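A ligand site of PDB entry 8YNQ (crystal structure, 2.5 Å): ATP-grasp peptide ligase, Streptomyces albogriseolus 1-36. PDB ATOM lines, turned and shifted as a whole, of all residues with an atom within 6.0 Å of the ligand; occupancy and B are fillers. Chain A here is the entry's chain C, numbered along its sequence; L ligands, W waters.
N of Asp 325 is in hydrogen-bond range of O of Glu 338 (3.1 Å). OE2 of Glu 338 is in hydrogen-bond range of ND2 of Asn 340 (3.2 Å). NZ of Lys 188 is in salt-bridge range of OE1 of Glu 245 (3.0 Å). NH2 of Arg 253 sits at hydrogen-bond distance from O of His 248, at 3.3 Å. O of Arg 253 lies within hydrogen-bond range of N of Leu 273, 2.6 Å away. The backbone carbonyl oxygen of Pro 210 sits at hydrogen-bond distance from the side-chain hydroxyl of Tyr 247 (2.7 Å). The side-chain carboxylate (OD1) of Asp 325 sits close to the side-chain amide oxygen (OD1) of Asn 323, at 3.0 Å. The side-chain carboxylate (OE2) of Glu 245 sits at hydrogen-bond distance from the side-chain hydroxyl (OG1) of Thr 160 (3.4 Å).
N of Gly 195 sits at hydrogen-bond distance from O5 of the ligand, at 2.4 Å. The side-chain carboxylate (OE2) of Glu 338 lies within hydrogen-bond range of a nitrogen (N1) of the ligand. NZ of Lys 188 is in salt-bridge range of O7 of the ligand, 2.9 Å away. The backbone NH of Gly 194 sits at hydrogen-bond distance from an oxygen (O1) of the ligand (2.9 Å). The guanidinium group (NE) of Arg 253 is in hydrogen-bond range of an oxygen (O12) of the ligand. An oxygen (O11) of the ligand is in hydrogen-bond range of the side-chain hydroxyl (OH) of Tyr 275, at 3.0 Å. The side-chain carboxylate of Asp 325 sits at hydrogen-bond distance from a nitrogen (N1) of the ligand. NZ of Lys 145 lies within salt-bridge range of O4 of the ligand. A nitrogen (N4) of the ligand lies within hydrogen-bond range of the backbone carbonyl oxygen (O) of Thr 246 (3.2 Å). OE1 of Glu 245 sits at hydrogen-bond distance from N4 of the ligand (3.2 Å). The backbone NH of His 248 sits at hydrogen-bond distance from a nitrogen (N5) of the ligand (3.2 Å). O2 of the ligand is in hydrogen-bond range of ND2 of Asn 340. O5 of the ligand lies within hydrogen-bond range of ND2 of Asn 198. NH2 of Arg 342 lies within salt-bridge range of O2 of the ligand (3.7 Å).
The backbone carbonyl oxygen (O) of Pro 210 lies close to an oxygen (O10) of the ligand, 3.0 Å away. Merely in contact with the ligand: Gly 193, Gly 211, Tyr 247, Ile 186, His 337, Ser 192 and Leu 273.
Water W1 lies within hydrogen-bond range of a ring nitrogen (ND1) of His 337 (2.4 Å), the side-chain carboxylate of Glu 245 (2.9 Å) and a nitrogen (N4) of the ligand (3.1 Å).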
ATOM      1  N   LYS A 145      12.690  25.701 -19.903  1.00  0.00           N
ATOM      2  CA  LYS A 145      12.430  24.604 -18.982  1.00  0.00           C
ATOM      3  C   LYS A 145      11.890  23.400 -19.742  1.00  0.00           C
ATOM      4  O   LYS A 145      12.399  22.284 -19.601  1.00  0.00           O
ATOM      5  CB  LYS A 145      11.444  25.057 -17.900  1.00  0.00           C
ATOM      6  CG  LYS A 145      12.031  26.060 -16.898  1.00  0.00           C
ATOM      7  CD  LYS A 145      12.393  25.401 -15.590  1.00  0.00           C
ATOM      8  CE  LYS A 145      13.547  26.120 -14.945  1.00  0.00           C
ATOM      9  NZ  LYS A 145      13.504  27.597 -15.196  1.00  0.00           N
ATOM     10  N   THR A 160      11.929  14.687 -12.024  1.00  0.00           N
ATOM     11  CA  THR A 160      10.728  14.577 -11.207  1.00  0.00           C
ATOM     12  C   THR A 160       9.509  14.415 -12.099  1.00  0.00           C
ATOM     13  O   THR A 160       9.459  14.998 -13.180  1.00  0.00           O
ATOM     14  CB  THR A 160      10.549  15.825 -10.360  1.00  0.00           C
ATOM     15  OG1 THR A 160      10.233  16.931 -11.225  1.00  0.00           O
ATOM     16  CG2 THR A 160      11.811  16.123  -9.586  1.00  0.00           C
ATOM     17  N   ILE A 186       5.215  22.237  -7.942  1.00  0.00           N
ATOM     18  CA  ILE A 186       5.803  23.500  -8.371  1.00  0.00           C
ATOM     19  C   ILE A 186       5.423  23.751  -9.815  1.00  0.00           C
ATOM     20  O   ILE A 186       5.236  22.824 -10.605  1.00  0.00           O
ATOM     21  CB  ILE A 186       7.331  23.502  -8.191  1.00  0.00           C
ATOM     22  CG1 ILE A 186       7.881  24.938  -8.302  1.00  0.00           C
ATOM     23  CG2 ILE A 186       7.953  22.510  -9.131  1.00  0.00           C
ATOM     24  CD1 ILE A 186       9.328  25.107  -7.812  1.00  0.00           C
ATOM     25  N   LYS A 188       6.247  26.446 -13.171  1.00  0.00           N
ATOM     26  CA  LYS A 188       7.260  27.402 -13.607  1.00  0.00           C
ATOM     27  C   LYS A 188       6.996  27.961 -15.008  1.00  0.00           C
ATOM     28  O   LYS A 188       6.509  27.254 -15.899  1.00  0.00           O
ATOM     29  CB  LYS A 188       8.650  26.753 -13.581  1.00  0.00           C
ATOM     30  CG  LYS A 188       8.892  25.745 -12.460  1.00  0.00           C
ATOM     31  CD  LYS A 188      10.367  25.311 -12.426  1.00  0.00           C
ATOM     32  CE  LYS A 188      10.563  23.987 -11.694  1.00  0.00           C
ATOM     33  NZ  LYS A 188      11.838  23.305 -12.055  1.00  0.00           N
ATOM     34  N   SER A 192      12.565  31.556 -17.845  1.00  0.00           N
ATOM     35  CA  SER A 192      12.742  32.501 -16.745  1.00  0.00           C
ATOM     36  C   SER A 192      13.935  32.052 -15.900  1.00  0.00           C
ATOM     37  O   SER A 192      14.702  31.153 -16.272  1.00  0.00           O
ATOM     38  CB  SER A 192      11.453  32.607 -15.927  1.00  0.00           C
ATOM     39  OG  SER A 192      11.371  33.861 -15.278  1.00  0.00           O
ATOM     40  N   GLY A 193      14.114  32.672 -14.736  1.00  0.00           N
ATOM     41  CA  GLY A 193      15.262  32.350 -13.921  1.00  0.00           C
ATOM     42  C   GLY A 193      15.171  32.976 -12.547  1.00  0.00           C
ATOM     43  O   GLY A 193      14.234  33.715 -12.229  1.00  0.00           O
ATOM     44  N   GLY A 194      16.180  32.662 -11.726  1.00  0.00           N
ATOM     45  CA  GLY A 194      16.274  33.226 -10.391  1.00  0.00           C
ATOM     46  C   GLY A 194      15.111  32.891  -9.485  1.00  0.00           C
ATOM     47  O   GLY A 194      14.921  33.581  -8.469  1.00  0.00           O
ATOM     48  N   GLY A 195      14.337  31.850  -9.802  1.00  0.00           N
ATOM     49  CA  GLY A 195      13.143  31.529  -9.036  1.00  0.00           C
ATOM     50  C   GLY A 195      12.042  32.555  -9.114  1.00  0.00           C
ATOM     51  O   GLY A 195      11.211  32.614  -8.216  1.00  0.00           O
ATOM     52  N   HIS A 196      12.018  33.368 -10.169  1.00  0.00           N
ATOM     53  CA  HIS A 196      10.998  34.396 -10.325  1.00  0.00           C
ATOM     54  C   HIS A 196       9.760  33.902 -11.054  1.00  0.00           C
ATOM     55  O   HIS A 196       8.727  34.570 -10.997  1.00  0.00           O
ATOM     56  CB  HIS A 196      11.540  35.598 -11.105  1.00  0.00           C
ATOM     57  CG  HIS A 196      12.865  36.076 -10.623  1.00  0.00           C
ATOM     58  ND1 HIS A 196      14.055  35.691 -11.190  1.00  0.00           N
ATOM     59  CD2 HIS A 196      13.188  36.935  -9.619  1.00  0.00           C
ATOM     60  CE1 HIS A 196      15.055  36.278 -10.560  1.00  0.00           C
ATOM     61  NE2 HIS A 196      14.555  37.040  -9.604  1.00  0.00           N
ATOM     62  N   GLY A 197       9.848  32.782 -11.747  1.00  0.00           N
ATOM     63  CA  GLY A 197       8.724  32.318 -12.526  1.00  0.00           C
ATOM     64  C   GLY A 197       8.061  31.112 -11.908  1.00  0.00           C
ATOM     65  O   GLY A 197       7.121  30.572 -12.472  1.00  0.00           O
ATOM     66  N   ASN A 198       8.557  30.679 -10.757  1.00  0.00           N
ATOM     67  CA  ASN A 198       8.109  29.444 -10.138  1.00  0.00           C
ATOM     68  C   ASN A 198       7.097  29.765  -9.059  1.00  0.00           C
ATOM     69  O   ASN A 198       7.366  30.563  -8.144  1.00  0.00           O
ATOM     70  CB  ASN A 198       9.268  28.655  -9.551  1.00  0.00           C
ATOM     71  CG  ASN A 198      10.471  28.637 -10.456  1.00  0.00           C
ATOM     72  OD1 ASN A 198      10.352  28.706 -11.681  1.00  0.00           O
ATOM     73  ND2 ASN A 198      11.657  28.548  -9.854  1.00  0.00           N
ATOM     74  N   PRO A 210      12.073  26.796  -1.306  1.00  0.00           N
ATOM     75  CA  PRO A 210      13.194  27.352  -2.069  1.00  0.00           C
ATOM     76  C   PRO A 210      12.924  27.361  -3.568  1.00  0.00           C
ATOM     77  O   PRO A 210      12.351  26.421  -4.121  1.00  0.00           O
ATOM     78  CB  PRO A 210      14.344  26.417  -1.712  1.00  0.00           C
ATOM     79  CG  PRO A 210      14.067  26.090  -0.306  1.00  0.00           C
ATOM     80  CD  PRO A 210      12.547  25.927  -0.218  1.00  0.00           C
ATOM     81  N   GLY A 211      13.336  28.452  -4.203  1.00  0.00           N
ATOM     82  CA  GLY A 211      13.193  28.570  -5.633  1.00  0.00           C
ATOM     83  C   GLY A 211      11.817  28.924  -6.141  1.00  0.00           C
ATOM     84  O   GLY A 211      11.449  28.494  -7.237  1.00  0.00           O
ATOM     85  N   THR A 212      11.040  29.704  -5.387  1.00  0.00           N
ATOM     86  CA  THR A 212       9.721  30.157  -5.825  1.00  0.00           C
ATOM     87  C   THR A 212       9.483  31.586  -5.362  1.00  0.00           C
ATOM     88  O   THR A 212      10.104  32.040  -4.398  1.00  0.00           O
ATOM     89  CB  THR A 212       8.609  29.275  -5.258  1.00  0.00           C
ATOM     90  OG1 THR A 212       8.517  29.508  -3.849  1.00  0.00           O
ATOM     91  CG2 THR A 212       8.866  27.803  -5.503  1.00  0.00           C
ATOM     92  N   GLU A 245       5.369  19.958 -11.936  1.00  0.00           N
ATOM     93  CA  GLU A 245       6.209  18.913 -11.361  1.00  0.00           C
ATOM     94  C   GLU A 245       5.887  18.673  -9.889  1.00  0.00           C
ATOM     95  O   GLU A 245       5.446  19.574  -9.171  1.00  0.00           O
ATOM     96  CB  GLU A 245       7.712  19.245 -11.444  1.00  0.00           C
ATOM     97  CG  GLU A 245       8.221  19.739 -12.758  1.00  0.00           C
ATOM     98  CD  GLU A 245       9.718  20.034 -12.699  1.00  0.00           C
ATOM     99  OE1 GLU A 245      10.086  20.866 -11.841  1.00  0.00           O
ATOM    100  OE2 GLU A 245      10.522  19.435 -13.492  1.00  0.00           O
ATOM    101  N   THR A 246       6.185  17.464  -9.437  1.00  0.00           N
ATOM    102  CA  THR A 246       6.209  17.158  -8.015  1.00  0.00           C
ATOM    103  C   THR A 246       7.331  17.936  -7.337  1.00  0.00           C
ATOM    104  O   THR A 246       8.488  17.850  -7.758  1.00  0.00           O
ATOM    105  CB  THR A 246       6.411  15.653  -7.813  1.00  0.00           C
ATOM    106  OG1 THR A 246       5.356  14.934  -8.470  1.00  0.00           O
ATOM    107  CG2 THR A 246       6.495  15.272  -6.326  1.00  0.00           C
ATOM    108  N   TYR A 247       7.014  18.695  -6.303  1.00  0.00           N
ATOM    109  CA  TYR A 247       8.029  19.395  -5.539  1.00  0.00           C
ATOM    110  C   TYR A 247       8.465  18.510  -4.379  1.00  0.00           C
ATOM    111  O   TYR A 247       7.629  18.054  -3.581  1.00  0.00           O
ATOM    112  CB  TYR A 247       7.504  20.727  -5.007  1.00  0.00           C
ATOM    113  CG  TYR A 247       8.608  21.646  -4.466  1.00  0.00           C
ATOM    114  CD1 TYR A 247       9.042  21.544  -3.144  1.00  0.00           C
ATOM    115  CD2 TYR A 247       9.231  22.580  -5.289  1.00  0.00           C
ATOM    116  CE1 TYR A 247      10.060  22.361  -2.664  1.00  0.00           C
ATOM    117  CE2 TYR A 247      10.229  23.407  -4.803  1.00  0.00           C
ATOM    118  CZ  TYR A 247      10.643  23.280  -3.490  1.00  0.00           C
ATOM    119  OH  TYR A 247      11.637  24.101  -3.011  1.00  0.00           O
ATOM    120  N   HIS A 248       9.771  18.290  -4.267  1.00  0.00           N
ATOM    121  CA  HIS A 248      10.354  17.478  -3.203  1.00  0.00           C
ATOM    122  C   HIS A 248      11.071  18.348  -2.168  1.00  0.00           C
ATOM    123  O   HIS A 248      11.633  19.395  -2.499  1.00  0.00           O
ATOM    124  CB  HIS A 248      11.359  16.464  -3.744  1.00  0.00           C
ATOM    125  CG  HIS A 248      10.762  15.397  -4.608  1.00  0.00           C
ATOM    126  ND1 HIS A 248      10.055  14.331  -4.094  1.00  0.00           N
ATOM    127  CD2 HIS A 248      10.795  15.223  -5.949  1.00  0.00           C
ATOM    128  CE1 HIS A 248       9.663  13.554  -5.087  1.00  0.00           C
ATOM    129  NE2 HIS A 248      10.104  14.068  -6.216  1.00  0.00           N
ATOM    130  N   ARG A 249      11.045  17.888  -0.909  1.00  0.00           N
ATOM    131  CA  ARG A 249      11.984  18.326   0.120  1.00  0.00           C
ATOM    132  C   ARG A 249      13.360  17.695  -0.132  1.00  0.00           C
ATOM    133  O   ARG A 249      13.456  16.576  -0.650  1.00  0.00           O
ATOM    134  CB  ARG A 249      11.467  17.919   1.501  1.00  0.00           C
ATOM    135  CG  ARG A 249      11.242  19.061   2.458  1.00  0.00           C
ATOM    136  CD  ARG A 249      10.121  20.003   1.998  1.00  0.00           C
ATOM    137  NE  ARG A 249      10.085  21.216   2.814  1.00  0.00           N
ATOM    138  CZ  ARG A 249       9.248  21.429   3.826  1.00  0.00           C
ATOM    139  NH1 ARG A 249       8.269  20.579   4.100  1.00  0.00           N
ATOM    140  NH2 ARG A 249       9.416  22.513   4.585  1.00  0.00           N
ATOM    141  N   ARG A 253      20.642  21.277  -2.142  1.00  0.00           N
ATOM    142  CA  ARG A 253      20.227  21.977  -3.355  1.00  0.00           C
ATOM    143  C   ARG A 253      21.498  22.477  -4.030  1.00  0.00           C
ATOM    144  O   ARG A 253      22.099  23.470  -3.604  1.00  0.00           O
ATOM    145  CB  ARG A 253      19.260  23.104  -3.045  1.00  0.00           C
ATOM    146  CG  ARG A 253      17.957  22.632  -2.386  1.00  0.00           C
ATOM    147  CD  ARG A 253      16.884  23.712  -2.411  1.00  0.00           C
ATOM    148  NE  ARG A 253      15.568  23.184  -2.781  1.00  0.00           N
ATOM    149  CZ  ARG A 253      14.805  22.504  -1.951  1.00  0.00           C
ATOM    150  NH1 ARG A 253      15.182  22.246  -0.711  1.00  0.00           N
ATOM    151  NH2 ARG A 253      13.635  22.023  -2.379  1.00  0.00           N
ATOM    152  N   PHE A 254      21.910  21.792  -5.093  1.00  0.00           N
ATOM    153  CA  PHE A 254      23.227  21.920  -5.665  1.00  0.00           C
ATOM    154  C   PHE A 254      23.127  22.260  -7.151  1.00  0.00           C
ATOM    155  O   PHE A 254      22.065  22.143  -7.775  1.00  0.00           O
ATOM    156  CB  PHE A 254      24.011  20.603  -5.480  1.00  0.00           C
ATOM    157  CG  PHE A 254      23.568  19.480  -6.395  1.00  0.00           C
ATOM    158  CD1 PHE A 254      24.037  19.390  -7.708  1.00  0.00           C
ATOM    159  CD2 PHE A 254      22.699  18.498  -5.938  1.00  0.00           C
ATOM    160  CE1 PHE A 254      23.621  18.375  -8.541  1.00  0.00           C
ATOM    161  CE2 PHE A 254      22.275  17.484  -6.765  1.00  0.00           C
ATOM    162  CZ  PHE A 254      22.735  17.415  -8.059  1.00  0.00           C
ATOM    163  N   LEU A 273      23.229  25.747  -2.991  1.00  0.00           N
ATOM    164  CA  LEU A 273      22.320  26.874  -3.102  1.00  0.00           C
ATOM    165  C   LEU A 273      21.653  27.102  -1.761  1.00  0.00           C
ATOM    166  O   LEU A 273      21.001  26.191  -1.222  1.00  0.00           O
ATOM    167  CB  LEU A 273      21.267  26.612  -4.182  1.00  0.00           C
ATOM    168  CG  LEU A 273      21.609  26.137  -5.599  1.00  0.00           C
ATOM    169  CD1 LEU A 273      20.565  25.134  -6.128  1.00  0.00           C
ATOM    170  CD2 LEU A 273      21.749  27.302  -6.564  1.00  0.00           C
ATOM    171  N   TYR A 275      19.027  29.093   0.684  1.00  0.00           N
ATOM    172  CA  TYR A 275      17.766  29.821   0.679  1.00  0.00           C
ATOM    173  C   TYR A 275      17.394  30.237   2.093  1.00  0.00           C
ATOM    174  O   TYR A 275      17.931  29.729   3.082  1.00  0.00           O
ATOM    175  CB  TYR A 275      16.638  28.987   0.053  1.00  0.00           C
ATOM    176  CG  TYR A 275      16.943  28.499  -1.326  1.00  0.00           C
ATOM    177  CD1 TYR A 275      17.811  27.436  -1.542  1.00  0.00           C
ATOM    178  CD2 TYR A 275      16.362  29.092  -2.430  1.00  0.00           C
ATOM    179  CE1 TYR A 275      18.089  26.977  -2.820  1.00  0.00           C
ATOM    180  CE2 TYR A 275      16.624  28.636  -3.714  1.00  0.00           C
ATOM    181  CZ  TYR A 275      17.495  27.577  -3.906  1.00  0.00           C
ATOM    182  OH  TYR A 275      17.776  27.132  -5.183  1.00  0.00           O
ATOM    183  N   ASN A 323      25.273  25.250 -16.812  1.00  0.00           N
ATOM    184  CA  ASN A 323      25.194  24.600 -15.518  1.00  0.00           C
ATOM    185  C   ASN A 323      23.882  23.842 -15.377  1.00  0.00           C
ATOM    186  O   ASN A 323      22.882  24.169 -16.005  1.00  0.00           O
ATOM    187  CB  ASN A 323      25.360  25.608 -14.389  1.00  0.00           C
ATOM    188  CG  ASN A 323      24.130  26.431 -14.198  1.00  0.00           C
ATOM    189  OD1 ASN A 323      23.236  26.042 -13.459  1.00  0.00           O
ATOM    190  ND2 ASN A 323      24.056  27.579 -14.884  1.00  0.00           N
ATOM    191  N   ASP A 325      21.173  22.227 -12.472  1.00  0.00           N
ATOM    192  CA  ASP A 325      20.669  22.339 -11.107  1.00  0.00           C
ATOM    193  C   ASP A 325      20.167  20.979 -10.643  1.00  0.00           C
ATOM    194  O   ASP A 325      19.743  20.166 -11.461  1.00  0.00           O
ATOM    195  CB  ASP A 325      19.502  23.346 -11.044  1.00  0.00           C
ATOM    196  CG  ASP A 325      19.927  24.803 -11.293  1.00  0.00           C
ATOM    197  OD1 ASP A 325      21.103  25.061 -11.660  1.00  0.00           O
ATOM    198  OD2 ASP A 325      19.067  25.722 -11.155  1.00  0.00           O
ATOM    199  N   GLY A 326      20.184  20.737  -9.331  1.00  0.00           N
ATOM    200  CA  GLY A 326      19.662  19.452  -8.872  1.00  0.00           C
ATOM    201  C   GLY A 326      19.493  19.342  -7.368  1.00  0.00           C
ATOM    202  O   GLY A 326      20.018  20.158  -6.598  1.00  0.00           O
ATOM    203  N   ILE A 327      18.778  18.283  -6.959  1.00  0.00           N
ATOM    204  CA  ILE A 327      18.530  17.979  -5.549  1.00  0.00           C
ATOM    205  C   ILE A 327      18.836  16.519  -5.250  1.00  0.00           C
ATOM    206  O   ILE A 327      18.721  15.640  -6.119  1.00  0.00           O
ATOM    207  CB  ILE A 327      17.073  18.280  -5.120  1.00  0.00           C
ATOM    208  CG1 ILE A 327      16.094  17.543  -6.060  1.00  0.00           C
ATOM    209  CG2 ILE A 327      16.819  19.787  -5.074  1.00  0.00           C
ATOM    210  CD1 ILE A 327      14.934  16.863  -5.358  1.00  0.00           C
ATOM    211  N   HIS A 337      16.878  19.644 -12.517  1.00  0.00           N
ATOM    212  CA  HIS A 337      15.801  20.617 -12.733  1.00  0.00           C
ATOM    213  C   HIS A 337      15.905  21.387 -14.043  1.00  0.00           C
ATOM    214  O   HIS A 337      14.893  21.589 -14.690  1.00  0.00           O
ATOM    215  CB  HIS A 337      15.740  21.638 -11.585  1.00  0.00           C
ATOM    216  CG  HIS A 337      15.674  21.002 -10.236  1.00  0.00           C
ATOM    217  ND1 HIS A 337      14.519  20.470  -9.710  1.00  0.00           N
ATOM    218  CD2 HIS A 337      16.648  20.741  -9.329  1.00  0.00           C
ATOM    219  CE1 HIS A 337      14.769  19.938  -8.534  1.00  0.00           C
ATOM    220  NE2 HIS A 337      16.057  20.081  -8.280  1.00  0.00           N
ATOM    221  N   GLU A 338      17.095  21.852 -14.417  1.00  0.00           N
ATOM    222  CA  GLU A 338      17.242  22.702 -15.601  1.00  0.00           C
ATOM    223  C   GLU A 338      18.728  22.822 -15.898  1.00  0.00           C
ATOM    224  O   GLU A 338      19.570  22.504 -15.056  1.00  0.00           O
ATOM    225  CB  GLU A 338      16.624  24.091 -15.381  1.00  0.00           C
ATOM    226  CG  GLU A 338      17.087  24.751 -14.083  1.00  0.00           C
ATOM    227  CD  GLU A 338      17.182  26.276 -14.130  1.00  0.00           C
ATOM    228  OE1 GLU A 338      16.536  26.923 -14.976  1.00  0.00           O
ATOM    229  OE2 GLU A 338      17.904  26.849 -13.282  1.00  0.00           O
ATOM    230  N   ASN A 340      21.180  26.152 -17.574  1.00  0.00           N
ATOM    231  CA  ASN A 340      21.219  27.537 -18.033  1.00  0.00           C
ATOM    232  C   ASN A 340      22.489  27.687 -18.861  1.00  0.00           C
ATOM    233  O   ASN A 340      23.602  27.602 -18.313  1.00  0.00           O
ATOM    234  CB  ASN A 340      21.187  28.560 -16.877  1.00  0.00           C
ATOM    235  CG  ASN A 340      20.348  28.104 -15.685  1.00  0.00           C
ATOM    236  OD1 ASN A 340      20.733  27.157 -14.992  1.00  0.00           O
ATOM    237  ND2 ASN A 340      19.219  28.768 -15.447  1.00  0.00           N
ATOM    238  N   ARG A 342      24.430  30.021 -19.774  1.00  0.00           N
ATOM    239  CA  ARG A 342      24.971  31.349 -19.484  1.00  0.00           C
ATOM    240  C   ARG A 342      25.861  31.283 -18.259  1.00  0.00           C
ATOM    241  O   ARG A 342      26.122  30.214 -17.719  1.00  0.00           O
ATOM    242  CB  ARG A 342      23.842  32.360 -19.257  1.00  0.00           C
ATOM    243  CG  ARG A 342      22.605  31.758 -18.626  1.00  0.00           C
ATOM    244  CD  ARG A 342      21.482  32.751 -18.569  1.00  0.00           C
ATOM    245  NE  ARG A 342      20.726  32.551 -17.340  1.00  0.00           N
ATOM    246  CZ  ARG A 342      19.609  31.854 -17.260  1.00  0.00           C
ATOM    247  NH1 ARG A 342      19.053  31.315 -18.334  1.00  0.00           N
ATOM    248  NH2 ARG A 342      19.048  31.670 -16.067  1.00  0.00           N
HETATM  249  P1  LIG L   1      17.905  29.623 -11.520  1.00  0.00           P
HETATM  250  O1  LIG L   1      17.766  30.593 -10.374  1.00  0.00           O
HETATM  251  O2  LIG L   1      17.613  30.315 -12.908  1.00  0.00           O
HETATM  252  O3  LIG L   1      19.381  29.014 -11.533  1.00  0.00           O
HETATM  253  P2  LIG L   1      15.271  28.738 -11.923  1.00  0.00           P
HETATM  254  O4  LIG L   1      15.355  29.276 -13.322  1.00  0.00           O
HETATM  255  O5  LIG L   1      14.642  29.766 -10.962  1.00  0.00           O
HETATM  256  N1  LIG L   1      16.813  28.350 -11.358  1.00  0.00           N
HETATM  257  P3  LIG L   1      14.805  26.193 -10.970  1.00  0.00           P
HETATM  258  O6  LIG L   1      16.032  25.525 -11.442  1.00  0.00           O
HETATM  259  O7  LIG L   1      13.562  25.305 -10.799  1.00  0.00           O
HETATM  260  O8  LIG L   1      14.413  27.424 -11.930  1.00  0.00           O
HETATM  261  O9  LIG L   1      15.227  26.865  -9.592  1.00  0.00           O
HETATM  262  C1  LIG L   1      14.354  26.885  -8.479  1.00  0.00           C
HETATM  263  C2  LIG L   1      14.989  26.176  -7.315  1.00  0.00           C
HETATM  264  O10 LIG L   1      13.940  25.616  -6.497  1.00  0.00           O
HETATM  265  C3  LIG L   1      15.939  25.018  -7.647  1.00  0.00           C
HETATM  266  O11 LIG L   1      17.285  25.453  -7.581  1.00  0.00           O
HETATM  267  C4  LIG L   1      15.669  24.022  -6.519  1.00  0.00           C
HETATM  268  O12 LIG L   1      16.347  24.435  -5.335  1.00  0.00           O
HETATM  269  C5  LIG L   1      14.185  24.252  -6.266  1.00  0.00           C
HETATM  270  N2  LIG L   1      13.283  23.470  -7.103  1.00  0.00           N
HETATM  271  C6  LIG L   1      12.817  23.765  -8.355  1.00  0.00           C
HETATM  272  N3  LIG L   1      11.997  22.866  -8.851  1.00  0.00           N
HETATM  273  C7  LIG L   1      11.889  21.927  -7.832  1.00  0.00           C
HETATM  274  C8  LIG L   1      11.157  20.716  -7.718  1.00  0.00           C
HETATM  275  N4  LIG L   1      10.358  20.232  -8.676  1.00  0.00           N
HETATM  276  N5  LIG L   1      11.281  20.019  -6.564  1.00  0.00           N
HETATM  277  C9  LIG L   1      12.078  20.489  -5.607  1.00  0.00           C
HETATM  278  N6  LIG L   1      12.812  21.607  -5.597  1.00  0.00           N
HETATM  279  C10 LIG L   1      12.672  22.284  -6.754  1.00  0.00           C
HETATM  280  O   HOH W   1      12.530  19.751 -10.869  1.00  0.00           O
